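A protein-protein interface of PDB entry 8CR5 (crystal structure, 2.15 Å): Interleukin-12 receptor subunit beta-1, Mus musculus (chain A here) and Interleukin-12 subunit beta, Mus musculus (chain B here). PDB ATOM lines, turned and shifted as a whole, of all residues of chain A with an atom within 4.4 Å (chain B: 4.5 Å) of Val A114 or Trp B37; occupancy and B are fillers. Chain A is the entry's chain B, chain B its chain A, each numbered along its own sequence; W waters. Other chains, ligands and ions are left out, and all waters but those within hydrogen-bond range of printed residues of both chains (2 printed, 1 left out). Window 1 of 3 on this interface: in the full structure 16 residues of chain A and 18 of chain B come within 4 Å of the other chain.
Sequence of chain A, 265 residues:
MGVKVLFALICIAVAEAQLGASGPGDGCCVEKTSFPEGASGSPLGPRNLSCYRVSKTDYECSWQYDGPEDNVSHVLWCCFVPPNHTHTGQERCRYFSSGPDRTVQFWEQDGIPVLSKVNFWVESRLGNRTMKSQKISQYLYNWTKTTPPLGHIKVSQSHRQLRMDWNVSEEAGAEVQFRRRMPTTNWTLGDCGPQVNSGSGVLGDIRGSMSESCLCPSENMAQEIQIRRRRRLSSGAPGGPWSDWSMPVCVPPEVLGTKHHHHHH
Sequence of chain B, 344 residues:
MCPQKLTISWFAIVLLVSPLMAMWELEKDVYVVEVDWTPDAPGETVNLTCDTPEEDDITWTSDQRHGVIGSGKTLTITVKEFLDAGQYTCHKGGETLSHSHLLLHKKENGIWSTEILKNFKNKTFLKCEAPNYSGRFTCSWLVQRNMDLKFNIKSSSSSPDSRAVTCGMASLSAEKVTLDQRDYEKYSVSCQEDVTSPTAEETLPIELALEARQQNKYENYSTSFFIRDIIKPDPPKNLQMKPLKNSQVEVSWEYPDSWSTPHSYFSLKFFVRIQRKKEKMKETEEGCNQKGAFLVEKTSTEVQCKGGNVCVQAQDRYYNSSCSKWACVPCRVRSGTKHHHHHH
N of Val A114 sits at hydrogen-bond distance from OE1 of Glu B81.
The backbone NH (N) of Leu A115 is in hydrogen-bond range of the side-chain carboxylate (OE2) of Glu B81, at 3.0 Å.
OE1 of Glu A108 is in salt-bridge range of NZ of Lys B106, at 2.7 Å.
The guanidinium group (NH1) of Arg A53 lies within salt-bridge range of the side-chain carboxylate (OE2) of Glu B108 (2.9 Å).
The backbone carbonyl oxygen (O) of Lys B107 lies within hydrogen-bond range of the backbone NH (N) of Trp B37, 3.2 Å away.
The side-chain amino group (NZ) of Lys B80 sits at hydrogen-bond distance from the backbone carbonyl oxygen (O) of Thr B38, at 2.7 Å.
NH1 of Arg A53 sits at hydrogen-bond distance from O of Tyr A141, 3.3 Å away.
O of Val A114 sits at hydrogen-bond distance from N of Tyr A141, at 3.1 Å.
Among the printed residues, merely in contact across the chains: Glu A108 with Trp B37 (3.8 Å), Glu A108 with Phe B82 (3.4 Å), Pro A113 with Glu B81 (3.2 Å), Val A114 with Trp B37 (3.7 Å), Leu A115 with Trp B37 (3.7 Å), Leu A115 with Thr B38 (3.9 Å), Ser A116 with Glu B81 (3.5 Å) and Tyr A141 with Trp B37 (3.7 Å).
Tyr A59 touches none of the printed residues of chain B.
Of the printed residues of chain B, Tyr A141 touches Trp B37 (3.7 Å).
Printed residues of chain A within 4 Å of Thr B38: Leu A115 (3.9 Å).
Lys B107 touches none of the printed residues of chain A.
The nearest residue of chain A that does not touch Trp B37 is Arg A53 (4.1 Å).
Of the 10 printed residues of chain A, 7 touch a printed residue of chain B.
Hydrophobic or aromatic side chains of chain A within 4 Å of the printed part of chain B: Pro A113, Val A114, Leu A115 and Tyr A141.
Printed residues of chain B that touch a printed residue of chain A: Trp B37, Thr B38, Glu B81, Phe B82, Lys B106 and Glu B108.
Hydrophobic or aromatic side chains of chain B within 4 Å of the printed part of chain A: Trp B37 and Phe B82.
Among the printed residues, Asp or Glu carboxylates within 4 Å of a Lys or Arg side-chain nitrogen of the other chain: Arg A53 with Glu B108 (2.9 Å) and Glu A108 with Lys B106 (2.7 Å).
Water W2 lies within hydrogen-bond range of the side-chain carboxylate of Glu B81, the backbone NH of Phe B82 and the backbone carbonyl oxygen of Glu A108.
Water W1 lies within hydrogen-bond range of OH of Tyr A59 (2.7 Å), OE1 of Glu A108 (2.8 Å) and NE1 of Trp B37 (3.2 Å).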
ATOM      1  N   ARG A  53     -23.867 -11.459 -28.951  1.00  0.00           N
ATOM      2  CA  ARG A  53     -24.918 -11.175 -27.982  1.00  0.00           C
ATOM      3  C   ARG A  53     -25.136  -9.669 -27.898  1.00  0.00           C
ATOM      4  O   ARG A  53     -24.174  -8.901 -27.820  1.00  0.00           O
ATOM      5  CB  ARG A  53     -24.530 -11.733 -26.612  1.00  0.00           C
ATOM      6  CG  ARG A  53     -25.675 -12.126 -25.698  1.00  0.00           C
ATOM      7  CD  ARG A  53     -25.134 -12.881 -24.484  1.00  0.00           C
ATOM      8  NE  ARG A  53     -26.118 -13.058 -23.422  1.00  0.00           N
ATOM      9  CZ  ARG A  53     -25.884 -13.714 -22.293  1.00  0.00           C
ATOM     10  NH1 ARG A  53     -24.708 -14.270 -22.048  1.00  0.00           N
ATOM     11  NH2 ARG A  53     -26.852 -13.813 -21.386  1.00  0.00           N
ATOM     12  N   TYR A  59     -29.764 -12.013 -29.466  1.00  0.00           N
ATOM     13  CA  TYR A  59     -28.557 -12.215 -30.253  1.00  0.00           C
ATOM     14  C   TYR A  59     -28.756 -11.624 -31.642  1.00  0.00           C
ATOM     15  O   TYR A  59     -29.874 -11.290 -32.046  1.00  0.00           O
ATOM     16  CB  TYR A  59     -28.197 -13.705 -30.345  1.00  0.00           C
ATOM     17  CG  TYR A  59     -27.851 -14.328 -29.012  1.00  0.00           C
ATOM     18  CD1 TYR A  59     -28.847 -14.702 -28.117  1.00  0.00           C
ATOM     19  CD2 TYR A  59     -26.528 -14.534 -28.644  1.00  0.00           C
ATOM     20  CE1 TYR A  59     -28.535 -15.264 -26.896  1.00  0.00           C
ATOM     21  CE2 TYR A  59     -26.206 -15.102 -27.426  1.00  0.00           C
ATOM     22  CZ  TYR A  59     -27.214 -15.462 -26.556  1.00  0.00           C
ATOM     23  OH  TYR A  59     -26.901 -16.024 -25.342  1.00  0.00           O
ATOM     24  N   GLU A 108     -32.658 -16.326 -27.096  1.00  0.00           N
ATOM     25  CA  GLU A 108     -32.216 -17.590 -26.516  1.00  0.00           C
ATOM     26  C   GLU A 108     -33.251 -18.703 -26.616  1.00  0.00           C
ATOM     27  O   GLU A 108     -32.887 -19.878 -26.492  1.00  0.00           O
ATOM     28  CB  GLU A 108     -31.834 -17.373 -25.050  1.00  0.00           C
ATOM     29  CG  GLU A 108     -32.990 -16.881 -24.192  1.00  0.00           C
ATOM     30  CD  GLU A 108     -32.583 -16.611 -22.757  1.00  0.00           C
ATOM     31  OE1 GLU A 108     -31.366 -16.567 -22.479  1.00  0.00           O
ATOM     32  OE2 GLU A 108     -33.481 -16.435 -21.909  1.00  0.00           O
ATOM     33  N   ILE A 112     -31.771 -22.091 -31.187  1.00  0.00           N
ATOM     34  CA  ILE A 112     -30.353 -22.185 -31.524  1.00  0.00           C
ATOM     35  C   ILE A 112     -29.557 -22.230 -30.224  1.00  0.00           C
ATOM     36  O   ILE A 112     -29.760 -21.365 -29.362  1.00  0.00           O
ATOM     37  CB  ILE A 112     -29.897 -21.004 -32.400  1.00  0.00           C
ATOM     38  CG1 ILE A 112     -30.425 -21.158 -33.828  1.00  0.00           C
ATOM     39  CG2 ILE A 112     -28.380 -20.899 -32.407  1.00  0.00           C
ATOM     40  CD1 ILE A 112     -29.976 -20.057 -34.765  1.00  0.00           C
ATOM     41  N   PRO A 113     -28.661 -23.200 -30.044  1.00  0.00           N
ATOM     42  CA  PRO A 113     -27.893 -23.265 -28.795  1.00  0.00           C
ATOM     43  C   PRO A 113     -26.932 -22.094 -28.674  1.00  0.00           C
ATOM     44  O   PRO A 113     -26.321 -21.662 -29.654  1.00  0.00           O
ATOM     45  CB  PRO A 113     -27.136 -24.595 -28.906  1.00  0.00           C
ATOM     46  CG  PRO A 113     -27.805 -25.349 -30.023  1.00  0.00           C
ATOM     47  CD  PRO A 113     -28.333 -24.308 -30.954  1.00  0.00           C
ATOM     48  N   VAL A 114     -26.805 -21.577 -27.453  1.00  0.00           N
ATOM     49  CA  VAL A 114     -25.864 -20.500 -27.159  1.00  0.00           C
ATOM     50  C   VAL A 114     -24.722 -20.945 -26.260  1.00  0.00           C
ATOM     51  O   VAL A 114     -23.765 -20.174 -26.079  1.00  0.00           O
ATOM     52  CB  VAL A 114     -26.575 -19.277 -26.542  1.00  0.00           C
ATOM     53  CG1 VAL A 114     -27.818 -18.922 -27.344  1.00  0.00           C
ATOM     54  CG2 VAL A 114     -26.925 -19.540 -25.085  1.00  0.00           C
ATOM     55  N   LEU A 115     -24.778 -22.151 -25.699  1.00  0.00           N
ATOM     56  CA  LEU A 115     -23.718 -22.665 -24.843  1.00  0.00           C
ATOM     57  C   LEU A 115     -22.928 -23.792 -25.497  1.00  0.00           C
ATOM     58  O   LEU A 115     -22.158 -24.473 -24.814  1.00  0.00           O
ATOM     59  CB  LEU A 115     -24.298 -23.139 -23.508  1.00  0.00           C
ATOM     60  CG  LEU A 115     -25.084 -22.105 -22.697  1.00  0.00           C
ATOM     61  CD1 LEU A 115     -25.718 -22.750 -21.474  1.00  0.00           C
ATOM     62  CD2 LEU A 115     -24.186 -20.944 -22.291  1.00  0.00           C
ATOM     63  N   SER A 116     -23.106 -24.017 -26.798  1.00  0.00           N
ATOM     64  CA  SER A 116     -22.352 -25.038 -27.510  1.00  0.00           C
ATOM     65  C   SER A 116     -21.982 -24.517 -28.891  1.00  0.00           C
ATOM     66  O   SER A 116     -22.515 -23.509 -29.365  1.00  0.00           O
ATOM     67  CB  SER A 116     -23.133 -26.355 -27.615  1.00  0.00           C
ATOM     68  OG  SER A 116     -24.524 -26.120 -27.742  1.00  0.00           O
ATOM     69  N   LEU A 140     -22.024 -18.565 -28.845  1.00  0.00           N
ATOM     70  CA  LEU A 140     -22.755 -17.309 -28.938  1.00  0.00           C
ATOM     71  C   LEU A 140     -22.805 -16.532 -27.634  1.00  0.00           C
ATOM     72  O   LEU A 140     -22.788 -15.301 -27.665  1.00  0.00           O
ATOM     73  CB  LEU A 140     -24.190 -17.563 -29.417  1.00  0.00           C
ATOM     74  CG  LEU A 140     -24.351 -17.972 -30.883  1.00  0.00           C
ATOM     75  CD1 LEU A 140     -25.791 -18.355 -31.182  1.00  0.00           C
ATOM     76  CD2 LEU A 140     -23.886 -16.857 -31.810  1.00  0.00           C
ATOM     77  N   TYR A 141     -22.847 -17.219 -26.491  1.00  0.00           N
ATOM     78  CA  TYR A 141     -23.099 -16.543 -25.222  1.00  0.00           C
ATOM     79  C   TYR A 141     -21.993 -15.556 -24.858  1.00  0.00           C
ATOM     80  O   TYR A 141     -22.270 -14.523 -24.238  1.00  0.00           O
ATOM     81  CB  TYR A 141     -23.290 -17.585 -24.115  1.00  0.00           C
ATOM     82  CG  TYR A 141     -22.002 -18.046 -23.483  1.00  0.00           C
ATOM     83  CD1 TYR A 141     -21.017 -18.664 -24.244  1.00  0.00           C
ATOM     84  CD2 TYR A 141     -21.766 -17.865 -22.125  1.00  0.00           C
ATOM     85  CE1 TYR A 141     -19.834 -19.080 -23.675  1.00  0.00           C
ATOM     86  CE2 TYR A 141     -20.586 -18.287 -21.546  1.00  0.00           C
ATOM     87  CZ  TYR A 141     -19.619 -18.882 -22.328  1.00  0.00           C
ATOM     88  OH  TYR A 141     -18.439 -19.302 -21.759  1.00  0.00           O
ATOM     89  N   VAL B  35     -29.896 -24.136 -14.202  1.00  0.00           N
ATOM     90  CA  VAL B  35     -28.781 -24.334 -15.119  1.00  0.00           C
ATOM     91  C   VAL B  35     -27.773 -23.208 -14.948  1.00  0.00           C
ATOM     92  O   VAL B  35     -28.148 -22.044 -14.762  1.00  0.00           O
ATOM     93  CB  VAL B  35     -29.253 -24.417 -16.587  1.00  0.00           C
ATOM     94  CG1 VAL B  35     -29.963 -25.735 -16.844  1.00  0.00           C
ATOM     95  CG2 VAL B  35     -30.157 -23.239 -16.927  1.00  0.00           C
ATOM     96  N   ASP B  36     -26.492 -23.561 -15.003  1.00  0.00           N
ATOM     97  CA  ASP B  36     -25.431 -22.570 -15.096  1.00  0.00           C
ATOM     98  C   ASP B  36     -25.227 -22.196 -16.557  1.00  0.00           C
ATOM     99  O   ASP B  36     -25.170 -23.069 -17.430  1.00  0.00           O
ATOM    100  CB  ASP B  36     -24.135 -23.115 -14.496  1.00  0.00           C
ATOM    101  CG  ASP B  36     -24.245 -23.374 -13.009  1.00  0.00           C
ATOM    102  OD1 ASP B  36     -24.389 -22.397 -12.243  1.00  0.00           O
ATOM    103  OD2 ASP B  36     -24.197 -24.555 -12.605  1.00  0.00           O
ATOM    104  N   TRP B  37     -25.127 -20.897 -16.825  1.00  0.00           N
ATOM    105  CA  TRP B  37     -25.034 -20.400 -18.197  1.00  0.00           C
ATOM    106  C   TRP B  37     -23.575 -20.372 -18.661  1.00  0.00           C
ATOM    107  O   TRP B  37     -23.014 -19.332 -19.006  1.00  0.00           O
ATOM    108  CB  TRP B  37     -25.695 -19.029 -18.295  1.00  0.00           C
ATOM    109  CG  TRP B  37     -26.473 -18.791 -19.564  1.00  0.00           C
ATOM    110  CD1 TRP B  37     -26.293 -17.771 -20.451  1.00  0.00           C
ATOM    111  CD2 TRP B  37     -27.549 -19.589 -20.085  1.00  0.00           C
ATOM    112  NE1 TRP B  37     -27.189 -17.880 -21.487  1.00  0.00           N
ATOM    113  CE2 TRP B  37     -27.971 -18.987 -21.286  1.00  0.00           C
ATOM    114  CE3 TRP B  37     -28.196 -20.751 -19.652  1.00  0.00           C
ATOM    115  CZ2 TRP B  37     -29.007 -19.508 -22.060  1.00  0.00           C
ATOM    116  CZ3 TRP B  37     -29.226 -21.267 -20.422  1.00  0.00           C
ATOM    117  CH2 TRP B  37     -29.620 -20.645 -21.612  1.00  0.00           C
ATOM    118  N   THR B  38     -22.960 -21.554 -18.642  1.00  0.00           N
ATOM    119  CA  THR B  38     -21.612 -21.789 -19.135  1.00  0.00           C
ATOM    120  C   THR B  38     -21.593 -23.028 -20.016  1.00  0.00           C
ATOM    121  O   THR B  38     -22.389 -23.951 -19.818  1.00  0.00           O
ATOM    122  CB  THR B  38     -20.598 -21.986 -17.995  1.00  0.00           C
ATOM    123  OG1 THR B  38     -20.654 -23.342 -17.530  1.00  0.00           O
ATOM    124  CG2 THR B  38     -20.879 -21.045 -16.839  1.00  0.00           C
ATOM    125  N   LYS B  80     -29.428 -28.793 -20.531  1.00  0.00           N
ATOM    126  CA  LYS B  80     -28.409 -27.758 -20.410  1.00  0.00           C
ATOM    127  C   LYS B  80     -28.934 -26.375 -20.756  1.00  0.00           C
ATOM    128  O   LYS B  80     -28.662 -25.415 -20.027  1.00  0.00           O
ATOM    129  CB  LYS B  80     -27.217 -28.093 -21.314  1.00  0.00           C
ATOM    130  CG  LYS B  80     -25.951 -27.334 -20.986  1.00  0.00           C
ATOM    131  CD  LYS B  80     -24.829 -27.759 -21.916  1.00  0.00           C
ATOM    132  CE  LYS B  80     -23.492 -27.217 -21.466  1.00  0.00           C
ATOM    133  NZ  LYS B  80     -23.622 -26.276 -20.315  1.00  0.00           N
ATOM    134  N   GLU B  81     -29.657 -26.237 -21.861  1.00  0.00           N
ATOM    135  CA  GLU B  81     -30.212 -24.944 -22.248  1.00  0.00           C
ATOM    136  C   GLU B  81     -31.580 -25.176 -22.885  1.00  0.00           C
ATOM    137  O   GLU B  81     -32.190 -26.241 -22.743  1.00  0.00           O
ATOM    138  CB  GLU B  81     -29.232 -24.171 -23.144  1.00  0.00           C
ATOM    139  CG  GLU B  81     -28.749 -24.900 -24.380  1.00  0.00           C
ATOM    140  CD  GLU B  81     -27.828 -24.032 -25.209  1.00  0.00           C
ATOM    141  OE1 GLU B  81     -28.254 -22.919 -25.584  1.00  0.00           O
ATOM    142  OE2 GLU B  81     -26.680 -24.451 -25.475  1.00  0.00           O
ATOM    143  N   PHE B  82     -32.077 -24.162 -23.601  1.00  0.00           N
ATOM    144  CA  PHE B  82     -33.513 -24.055 -23.838  1.00  0.00           C
ATOM    145  C   PHE B  82     -34.024 -25.056 -24.864  1.00  0.00           C
ATOM    146  O   PHE B  82     -35.207 -25.414 -24.832  1.00  0.00           O
ATOM    147  CB  PHE B  82     -33.867 -22.629 -24.259  1.00  0.00           C
ATOM    148  CG  PHE B  82     -34.112 -21.710 -23.100  1.00  0.00           C
ATOM    149  CD1 PHE B  82     -35.252 -21.845 -22.328  1.00  0.00           C
ATOM    150  CD2 PHE B  82     -33.200 -20.719 -22.776  1.00  0.00           C
ATOM    151  CE1 PHE B  82     -35.482 -21.007 -21.256  1.00  0.00           C
ATOM    152  CE2 PHE B  82     -33.428 -19.876 -21.704  1.00  0.00           C
ATOM    153  CZ  PHE B  82     -34.571 -20.022 -20.945  1.00  0.00           C
ATOM    154  N   LYS B 106     -32.288 -19.696 -15.119  1.00  0.00           N
ATOM    155  CA  LYS B 106     -30.924 -19.360 -15.504  1.00  0.00           C
ATOM    156  C   LYS B 106     -30.154 -18.792 -14.316  1.00  0.00           C
ATOM    157  O   LYS B 106     -30.647 -17.908 -13.611  1.00  0.00           O
ATOM    158  CB  LYS B 106     -30.931 -18.349 -16.651  1.00  0.00           C
ATOM    159  CG  LYS B 106     -31.146 -18.957 -18.026  1.00  0.00           C
ATOM    160  CD  LYS B 106     -30.603 -18.050 -19.120  1.00  0.00           C
ATOM    161  CE  LYS B 106     -31.231 -16.671 -19.063  1.00  0.00           C
ATOM    162  NZ  LYS B 106     -30.627 -15.733 -20.055  1.00  0.00           N
ATOM    163  N   LYS B 107     -28.942 -19.293 -14.103  1.00  0.00           N
ATOM    164  CA  LYS B 107     -28.009 -18.745 -13.119  1.00  0.00           C
ATOM    165  C   LYS B 107     -26.719 -18.429 -13.865  1.00  0.00           C
ATOM    166  O   LYS B 107     -25.911 -19.326 -14.121  1.00  0.00           O
ATOM    167  CB  LYS B 107     -27.776 -19.747 -12.000  1.00  0.00           C
ATOM    168  CG  LYS B 107     -27.062 -19.269 -10.788  1.00  0.00           C
ATOM    169  CD  LYS B 107     -27.025 -20.371  -9.751  1.00  0.00           C
ATOM    170  CE  LYS B 107     -26.512 -19.736  -8.453  1.00  0.00           C
ATOM    171  NZ  LYS B 107     -26.415 -20.520  -7.153  1.00  0.00           N
ATOM    172  N   GLU B 108     -26.523 -17.161 -14.213  1.00  0.00           N
ATOM    173  CA  GLU B 108     -25.371 -16.723 -14.991  1.00  0.00           C
ATOM    174  C   GLU B 108     -24.452 -15.884 -14.118  1.00  0.00           C
ATOM    175  O   GLU B 108     -24.887 -14.883 -13.536  1.00  0.00           O
ATOM    176  CB  GLU B 108     -25.804 -15.918 -16.215  1.00  0.00           C
ATOM    177  CG  GLU B 108     -24.633 -15.397 -17.029  1.00  0.00           C
ATOM    178  CD  GLU B 108     -25.038 -14.953 -18.419  1.00  0.00           C
ATOM    179  OE1 GLU B 108     -26.251 -14.784 -18.661  1.00  0.00           O
ATOM    180  OE2 GLU B 108     -24.143 -14.764 -19.271  1.00  0.00           O
HETATM  181  O   HOH W   1     -28.794 -15.905 -23.458  1.00  0.00           O
HETATM  182  O   HOH W   2     -30.531 -21.730 -24.905  1.00  0.00           O
